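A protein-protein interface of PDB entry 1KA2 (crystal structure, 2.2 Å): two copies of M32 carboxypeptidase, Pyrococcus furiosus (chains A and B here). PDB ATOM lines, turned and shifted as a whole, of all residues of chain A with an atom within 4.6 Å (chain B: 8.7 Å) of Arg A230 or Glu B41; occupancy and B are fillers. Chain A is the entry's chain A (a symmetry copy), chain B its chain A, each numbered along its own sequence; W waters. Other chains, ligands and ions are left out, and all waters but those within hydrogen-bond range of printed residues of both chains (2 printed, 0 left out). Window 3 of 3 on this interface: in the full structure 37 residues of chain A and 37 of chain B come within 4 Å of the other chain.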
ATOM      1  N   PRO A 226     -17.648 -14.838   9.243  1.00  0.00           N
ATOM      2  CA  PRO A 226     -18.537 -13.669   9.178  1.00  0.00           C
ATOM      3  C   PRO A 226     -19.145 -13.293   7.820  1.00  0.00           C
ATOM      4  O   PRO A 226     -18.835 -12.235   7.267  1.00  0.00           O
ATOM      5  CB  PRO A 226     -17.665 -12.561   9.765  1.00  0.00           C
ATOM      6  CG  PRO A 226     -16.322 -12.901   9.205  1.00  0.00           C
ATOM      7  CD  PRO A 226     -16.239 -14.415   9.377  1.00  0.00           C
ATOM      8  N   GLY A 228     -21.531 -12.004   4.839  1.00  0.00           N
ATOM      9  CA  GLY A 228     -22.334 -10.807   4.650  1.00  0.00           C
ATOM     10  C   GLY A 228     -21.899  -9.605   5.463  1.00  0.00           C
ATOM     11  O   GLY A 228     -22.356  -8.488   5.232  1.00  0.00           O
ATOM     12  N   THR A 229     -21.006  -9.822   6.420  1.00  0.00           N
ATOM     13  CA  THR A 229     -20.532  -8.728   7.242  1.00  0.00           C
ATOM     14  C   THR A 229     -19.073  -8.366   6.919  1.00  0.00           C
ATOM     15  O   THR A 229     -18.740  -7.195   6.738  1.00  0.00           O
ATOM     16  CB  THR A 229     -20.689  -9.089   8.740  1.00  0.00           C
ATOM     17  OG1 THR A 229     -20.640  -7.893   9.523  1.00  0.00           O
ATOM     18  CG2 THR A 229     -19.575 -10.017   9.197  1.00  0.00           C
ATOM     19  N   ARG A 230     -18.209  -9.379   6.847  1.00  0.00           N
ATOM     20  CA  ARG A 230     -16.798  -9.192   6.537  1.00  0.00           C
ATOM     21  C   ARG A 230     -16.292 -10.239   5.538  1.00  0.00           C
ATOM     22  O   ARG A 230     -15.130 -10.226   5.155  1.00  0.00           O
ATOM     23  CB  ARG A 230     -15.961  -9.265   7.817  1.00  0.00           C
ATOM     24  CG  ARG A 230     -15.993  -7.991   8.647  1.00  0.00           C
ATOM     25  CD  ARG A 230     -15.289  -8.150   9.980  1.00  0.00           C
ATOM     26  NE  ARG A 230     -14.459  -6.981  10.247  1.00  0.00           N
ATOM     27  CZ  ARG A 230     -14.313  -6.421  11.440  1.00  0.00           C
ATOM     28  NH1 ARG A 230     -14.948  -6.924  12.486  1.00  0.00           N
ATOM     29  NH2 ARG A 230     -13.529  -5.366  11.589  1.00  0.00           N
ATOM     30  N   ALA A 231     -17.160 -11.142   5.100  1.00  0.00           N
ATOM     31  CA  ALA A 231     -16.703 -12.165   4.173  1.00  0.00           C
ATOM     32  C   ALA A 231     -17.774 -12.728   3.270  1.00  0.00           C
ATOM     33  O   ALA A 231     -18.975 -12.530   3.491  1.00  0.00           O
ATOM     34  CB  ALA A 231     -16.037 -13.307   4.956  1.00  0.00           C
ATOM     35  N   ILE A 246      -9.174  -5.844   5.663  1.00  0.00           N
ATOM     36  CA  ILE A 246      -9.286  -6.582   6.921  1.00  0.00           C
ATOM     37  C   ILE A 246     -10.756  -6.905   7.204  1.00  0.00           C
ATOM     38  O   ILE A 246     -11.078  -7.907   7.831  1.00  0.00           O
ATOM     39  CB  ILE A 246      -8.717  -5.750   8.100  1.00  0.00           C
ATOM     40  CG1 ILE A 246      -7.210  -5.552   7.913  1.00  0.00           C
ATOM     41  CG2 ILE A 246      -9.013  -6.441   9.427  1.00  0.00           C
ATOM     42  CD1 ILE A 246      -6.558  -4.684   8.991  1.00  0.00           C
ATOM     43  N   ARG A 247     -11.648  -6.049   6.726  1.00  0.00           N
ATOM     44  CA  ARG A 247     -13.074  -6.233   6.940  1.00  0.00           C
ATOM     45  C   ARG A 247     -13.768  -6.716   5.678  1.00  0.00           C
ATOM     46  O   ARG A 247     -14.984  -6.552   5.541  1.00  0.00           O
ATOM     47  CB  ARG A 247     -13.712  -4.916   7.395  1.00  0.00           C
ATOM     48  CG  ARG A 247     -13.140  -4.358   8.703  1.00  0.00           C
ATOM     49  CD  ARG A 247     -13.764  -2.996   9.053  1.00  0.00           C
ATOM     50  NE  ARG A 247     -13.170  -2.385  10.245  1.00  0.00           N
ATOM     51  CZ  ARG A 247     -13.502  -1.180  10.706  1.00  0.00           C
ATOM     52  NH1 ARG A 247     -14.417  -0.462  10.078  1.00  0.00           N
ATOM     53  NH2 ARG A 247     -12.924  -0.694  11.794  1.00  0.00           N
ATOM     54  N   ASP A 248     -13.007  -7.292   4.751  1.00  0.00           N
ATOM     55  CA  ASP A 248     -13.587  -7.797   3.510  1.00  0.00           C
ATOM     56  C   ASP A 248     -12.678  -8.881   2.947  1.00  0.00           C
ATOM     57  O   ASP A 248     -11.780  -8.587   2.170  1.00  0.00           O
ATOM     58  CB  ASP A 248     -13.737  -6.658   2.485  1.00  0.00           C
ATOM     59  CG  ASP A 248     -14.589  -7.050   1.292  1.00  0.00           C
ATOM     60  OD1 ASP A 248     -14.947  -8.238   1.174  1.00  0.00           O
ATOM     61  OD2 ASP A 248     -14.910  -6.167   0.461  1.00  0.00           O
ATOM     62  N   VAL A 249     -12.912 -10.129   3.343  1.00  0.00           N
ATOM     63  CA  VAL A 249     -12.091 -11.246   2.880  1.00  0.00           C
ATOM     64  C   VAL A 249     -13.005 -12.280   2.248  1.00  0.00           C
ATOM     65  O   VAL A 249     -14.023 -12.661   2.828  1.00  0.00           O
ATOM     66  CB  VAL A 249     -11.299 -11.874   4.052  1.00  0.00           C
ATOM     67  CG1 VAL A 249     -10.390 -12.996   3.542  1.00  0.00           C
ATOM     68  CG2 VAL A 249     -10.480 -10.798   4.743  1.00  0.00           C
ATOM     69  N   LEU A 278      -8.497 -12.155   8.167  1.00  0.00           N
ATOM     70  CA  LEU A 278      -9.617 -11.632   8.928  1.00  0.00           C
ATOM     71  C   LEU A 278      -9.167 -11.207  10.324  1.00  0.00           C
ATOM     72  O   LEU A 278      -9.615 -10.187  10.842  1.00  0.00           O
ATOM     73  CB  LEU A 278     -10.691 -12.717   9.034  1.00  0.00           C
ATOM     74  CG  LEU A 278     -12.122 -12.394   8.595  1.00  0.00           C
ATOM     75  CD1 LEU A 278     -12.110 -11.501   7.397  1.00  0.00           C
ATOM     76  CD2 LEU A 278     -12.871 -13.693   8.286  1.00  0.00           C
ATOM     77  N   GLU A 282      -6.380  -4.185  13.088  1.00  0.00           N
ATOM     78  CA  GLU A 282      -6.899  -3.001  12.396  1.00  0.00           C
ATOM     79  C   GLU A 282      -6.112  -1.702  12.578  1.00  0.00           C
ATOM     80  O   GLU A 282      -6.357  -0.725  11.874  1.00  0.00           O
ATOM     81  CB  GLU A 282      -8.364  -2.759  12.766  1.00  0.00           C
ATOM     82  CG  GLU A 282      -9.286  -3.920  12.416  1.00  0.00           C
ATOM     83  CD  GLU A 282     -10.752  -3.534  12.474  1.00  0.00           C
ATOM     84  OE1 GLU A 282     -11.106  -2.624  13.252  1.00  0.00           O
ATOM     85  OE2 GLU A 282     -11.552  -4.143  11.743  1.00  0.00           O
ATOM     86  N   ASN B  37     -22.074  -7.033  -4.130  1.00  0.00           N
ATOM     87  CA  ASN B  37     -21.493  -8.132  -3.356  1.00  0.00           C
ATOM     88  C   ASN B  37     -20.867  -7.860  -1.997  1.00  0.00           C
ATOM     89  O   ASN B  37     -20.975  -8.686  -1.091  1.00  0.00           O
ATOM     90  CB  ASN B  37     -20.439  -8.840  -4.208  1.00  0.00           C
ATOM     91  CG  ASN B  37     -20.970  -9.263  -5.556  1.00  0.00           C
ATOM     92  OD1 ASN B  37     -22.015  -9.883  -5.643  1.00  0.00           O
ATOM     93  ND2 ASN B  37     -20.242  -8.936  -6.617  1.00  0.00           N
ATOM     94  N   MET B  38     -20.199  -6.720  -1.879  1.00  0.00           N
ATOM     95  CA  MET B  38     -19.464  -6.330  -0.678  1.00  0.00           C
ATOM     96  C   MET B  38     -20.083  -6.571   0.691  1.00  0.00           C
ATOM     97  O   MET B  38     -21.213  -6.171   0.961  1.00  0.00           O
ATOM     98  CB  MET B  38     -19.060  -4.848  -0.773  1.00  0.00           C
ATOM     99  CG  MET B  38     -18.008  -4.425   0.246  1.00  0.00           C
ATOM    100  SD  MET B  38     -17.720  -2.653   0.331  1.00  0.00           S
ATOM    101  CE  MET B  38     -19.294  -2.103   1.046  1.00  0.00           C
ATOM    102  N   PRO B  39     -19.351  -7.271   1.573  1.00  0.00           N
ATOM    103  CA  PRO B  39     -19.903  -7.509   2.916  1.00  0.00           C
ATOM    104  C   PRO B  39     -20.023  -6.120   3.503  1.00  0.00           C
ATOM    105  O   PRO B  39     -19.148  -5.288   3.278  1.00  0.00           O
ATOM    106  CB  PRO B  39     -18.826  -8.317   3.644  1.00  0.00           C
ATOM    107  CG  PRO B  39     -17.847  -8.736   2.598  1.00  0.00           C
ATOM    108  CD  PRO B  39     -18.231  -8.174   1.264  1.00  0.00           C
ATOM    109  N   LYS B  40     -21.065  -5.868   4.280  1.00  0.00           N
ATOM    110  CA  LYS B  40     -21.301  -4.523   4.807  1.00  0.00           C
ATOM    111  C   LYS B  40     -20.146  -3.773   5.431  1.00  0.00           C
ATOM    112  O   LYS B  40     -19.932  -2.604   5.143  1.00  0.00           O
ATOM    113  CB  LYS B  40     -22.476  -4.540   5.783  1.00  0.00           C
ATOM    114  CG  LYS B  40     -23.792  -5.099   5.222  1.00  0.00           C
ATOM    115  CD  LYS B  40     -24.537  -4.150   4.245  1.00  0.00           C
ATOM    116  CE  LYS B  40     -25.889  -4.739   3.766  1.00  0.00           C
ATOM    117  NZ  LYS B  40     -26.575  -3.794   2.821  1.00  0.00           N
ATOM    118  N   GLU B  41     -19.393  -4.431   6.290  1.00  0.00           N
ATOM    119  CA  GLU B  41     -18.285  -3.754   6.921  1.00  0.00           C
ATOM    120  C   GLU B  41     -17.095  -3.448   6.003  1.00  0.00           C
ATOM    121  O   GLU B  41     -16.148  -2.781   6.411  1.00  0.00           O
ATOM    122  CB  GLU B  41     -17.806  -4.528   8.166  1.00  0.00           C
ATOM    123  CG  GLU B  41     -18.731  -4.508   9.362  1.00  0.00           C
ATOM    124  CD  GLU B  41     -18.069  -5.109  10.613  1.00  0.00           C
ATOM    125  OE1 GLU B  41     -17.179  -4.451  11.197  1.00  0.00           O
ATOM    126  OE2 GLU B  41     -18.425  -6.242  10.999  1.00  0.00           O
ATOM    127  N   GLY B  42     -17.116  -3.918   4.766  1.00  0.00           N
ATOM    128  CA  GLY B  42     -15.989  -3.610   3.899  1.00  0.00           C
ATOM    129  C   GLY B  42     -16.019  -2.183   3.361  1.00  0.00           C
ATOM    130  O   GLY B  42     -15.123  -1.758   2.634  1.00  0.00           O
ATOM    131  N   ILE B  43     -17.040  -1.428   3.750  1.00  0.00           N
ATOM    132  CA  ILE B  43     -17.218  -0.058   3.261  1.00  0.00           C
ATOM    133  C   ILE B  43     -16.097   0.933   3.549  1.00  0.00           C
ATOM    134  O   ILE B  43     -15.742   1.723   2.685  1.00  0.00           O
ATOM    135  CB  ILE B  43     -18.569   0.550   3.771  1.00  0.00           C
ATOM    136  CG1 ILE B  43     -18.785   1.951   3.183  1.00  0.00           C
ATOM    137  CG2 ILE B  43     -18.572   0.621   5.295  1.00  0.00           C
ATOM    138  CD1 ILE B  43     -19.125   1.968   1.709  1.00  0.00           C
ATOM    139  N   LEU B  44     -15.520   0.912   4.743  1.00  0.00           N
ATOM    140  CA  LEU B  44     -14.462   1.876   5.010  1.00  0.00           C
ATOM    141  C   LEU B  44     -13.258   1.694   4.089  1.00  0.00           C
ATOM    142  O   LEU B  44     -12.727   2.664   3.568  1.00  0.00           O
ATOM    143  CB  LEU B  44     -13.989   1.811   6.459  1.00  0.00           C
ATOM    144  CG  LEU B  44     -12.781   2.724   6.709  1.00  0.00           C
ATOM    145  CD1 LEU B  44     -13.143   4.169   6.353  1.00  0.00           C
ATOM    146  CD2 LEU B  44     -12.339   2.627   8.163  1.00  0.00           C
ATOM    147  N   GLU B  45     -12.830   0.452   3.888  1.00  0.00           N
ATOM    148  CA  GLU B  45     -11.673   0.198   3.045  1.00  0.00           C
ATOM    149  C   GLU B  45     -12.000   0.418   1.568  1.00  0.00           C
ATOM    150  O   GLU B  45     -11.170   0.923   0.812  1.00  0.00           O
ATOM    151  CB  GLU B  45     -11.136  -1.208   3.338  1.00  0.00           C
ATOM    152  CG  GLU B  45     -10.564  -1.281   4.769  1.00  0.00           C
ATOM    153  CD  GLU B  45     -10.341  -2.697   5.277  1.00  0.00           C
ATOM    154  OE1 GLU B  45     -11.340  -3.422   5.435  1.00  0.00           O
ATOM    155  OE2 GLU B  45      -9.171  -3.080   5.530  1.00  0.00           O
ATOM    156  N   ARG B  46     -13.217   0.070   1.162  1.00  0.00           N
ATOM    157  CA  ARG B  46     -13.632   0.302  -0.213  1.00  0.00           C
ATOM    158  C   ARG B  46     -13.594   1.812  -0.469  1.00  0.00           C
ATOM    159  O   ARG B  46     -13.036   2.264  -1.473  1.00  0.00           O
ATOM    160  CB  ARG B  46     -15.047  -0.241  -0.444  1.00  0.00           C
ATOM    161  CG  ARG B  46     -15.626  -0.012  -1.859  1.00  0.00           C
ATOM    162  CD  ARG B  46     -14.672  -0.476  -2.960  1.00  0.00           C
ATOM    163  NE  ARG B  46     -14.259  -1.849  -2.722  1.00  0.00           N
ATOM    164  CZ  ARG B  46     -14.973  -2.925  -3.032  1.00  0.00           C
ATOM    165  NH1 ARG B  46     -16.155  -2.801  -3.625  1.00  0.00           N
ATOM    166  NH2 ARG B  46     -14.518  -4.129  -2.701  1.00  0.00           N
ATOM    167  N   SER B  47     -14.143   2.584   0.467  1.00  0.00           N
ATOM    168  CA  SER B  47     -14.212   4.047   0.349  1.00  0.00           C
ATOM    169  C   SER B  47     -12.860   4.730   0.194  1.00  0.00           C
ATOM    170  O   SER B  47     -12.694   5.585  -0.672  1.00  0.00           O
ATOM    171  CB  SER B  47     -14.948   4.652   1.560  1.00  0.00           C
ATOM    172  OG  SER B  47     -14.050   4.894   2.637  1.00  0.00           O
HETATM  173  O   HOH W   1     -16.148  -0.685   7.663  1.00  0.00           O
HETATM  174  O   HOH W   2     -14.075  -3.901   0.453  1.00  0.00           O
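The guanidinium group (NH2) of Arg B46 lies within salt-bridge range of the side-chain carboxylate (OD2) of Asp A248, 3.8 Å away. The backbone NH (N) of Gly B42 lies within hydrogen-bond range of the backbone carbonyl oxygen (O) of Arg A247 (3.5 Å). N of Lys B40 is in hydrogen-bond range of O of Gly A228, at 3.1 Å. The side-chain carboxylate of Glu B45 is in hydrogen-bond range of the backbone NH of Arg A247 (2.9 Å). N of Glu B41 lies within hydrogen-bond range of O of Thr A229, 2.9 Å away. NH1 of Arg A230 is in salt-bridge range of OE1 of Glu B41 (3.6 Å). The side-chain carboxylate (OE2) of Glu B45 sits at hydrogen-bond distance from the backbone NH (N) of Ile A246 (2.8 Å).
The backbone carbonyl oxygen of Arg A230 lies within hydrogen-bond range of the backbone NH of Val A249. N of Ala A231 lies within hydrogen-bond range of O of Pro A226 (2.9 Å). SD of Met B38 sits close to N of Ile B43 (3.7 Å). The guanidinium group of Arg A247 is in salt-bridge range of the side-chain carboxylate of Glu A282.
Among the printed residues, pairs that only touch across the chains: Gly A228 with Pro B39, Thr A229 with Pro B39, Thr A229 with Lys B40, Arg A230 with Pro B39, Ala A231 with Pro B39, Arg A247 with Glu B41, Asp A248 with Met B38 and Asp A248 with Pro B39.
Printed residues of chain B within 4 Å of Arg A230: Pro B39 and Glu B41. Glu B41 touches three residues of chain A. Printed residues of chain B within 4 Å of Thr A229: Pro B39, Lys B40 and Glu B41. Printed residues of chain A within 4 Å of Lys B40: Gly A228 and Thr A229. Of the printed residues of chain A, Met B38 touches Asp A248. Leu B44 touches none of the printed residues of chain A. Val A249 touches none of the printed residues of chain B. The nearest printed residue of chain A that does not touch Glu B41 is Gly A228 (5.1 Å).
Of the 11 printed residues of chain A, 7 touch a printed residue of chain B. Printed residues of chain A that touch a printed residue of chain B: Gly A228, Thr A229, Arg A230, Ala A231, Ile A246, Arg A247 and Asp A248. Along chain A the printed residues that touch a printed residue of chain B span positions 228 to 248. Printed residues of chain B that touch a printed residue of chain A: Met B38, Pro B39, Lys B40, Glu B41, Gly B42, Glu B45 and Arg B46. Hydrophobic or aromatic side chains of chain B that line the printed part of chain A: Met B38 and Pro B39. Among the printed residues, 15 pairs touch across the chains.
No position is printed for both chains. Of the 15 pairs that touch across the chains among the printed residues, none has its exchanged pair printed and touching as well.
Water W2 lies within hydrogen-bond range of the side-chain carboxylate (OD2) of Asp A248, the guanidinium group (NH2) of Arg B46 and the backbone carbonyl oxygen (O) of Gly B42. Water W1 lies within hydrogen-bond range of the backbone carbonyl oxygen (O) of Glu B41, the guanidinium group (NH1) of Arg A247 and the backbone NH (N) of Leu B44.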
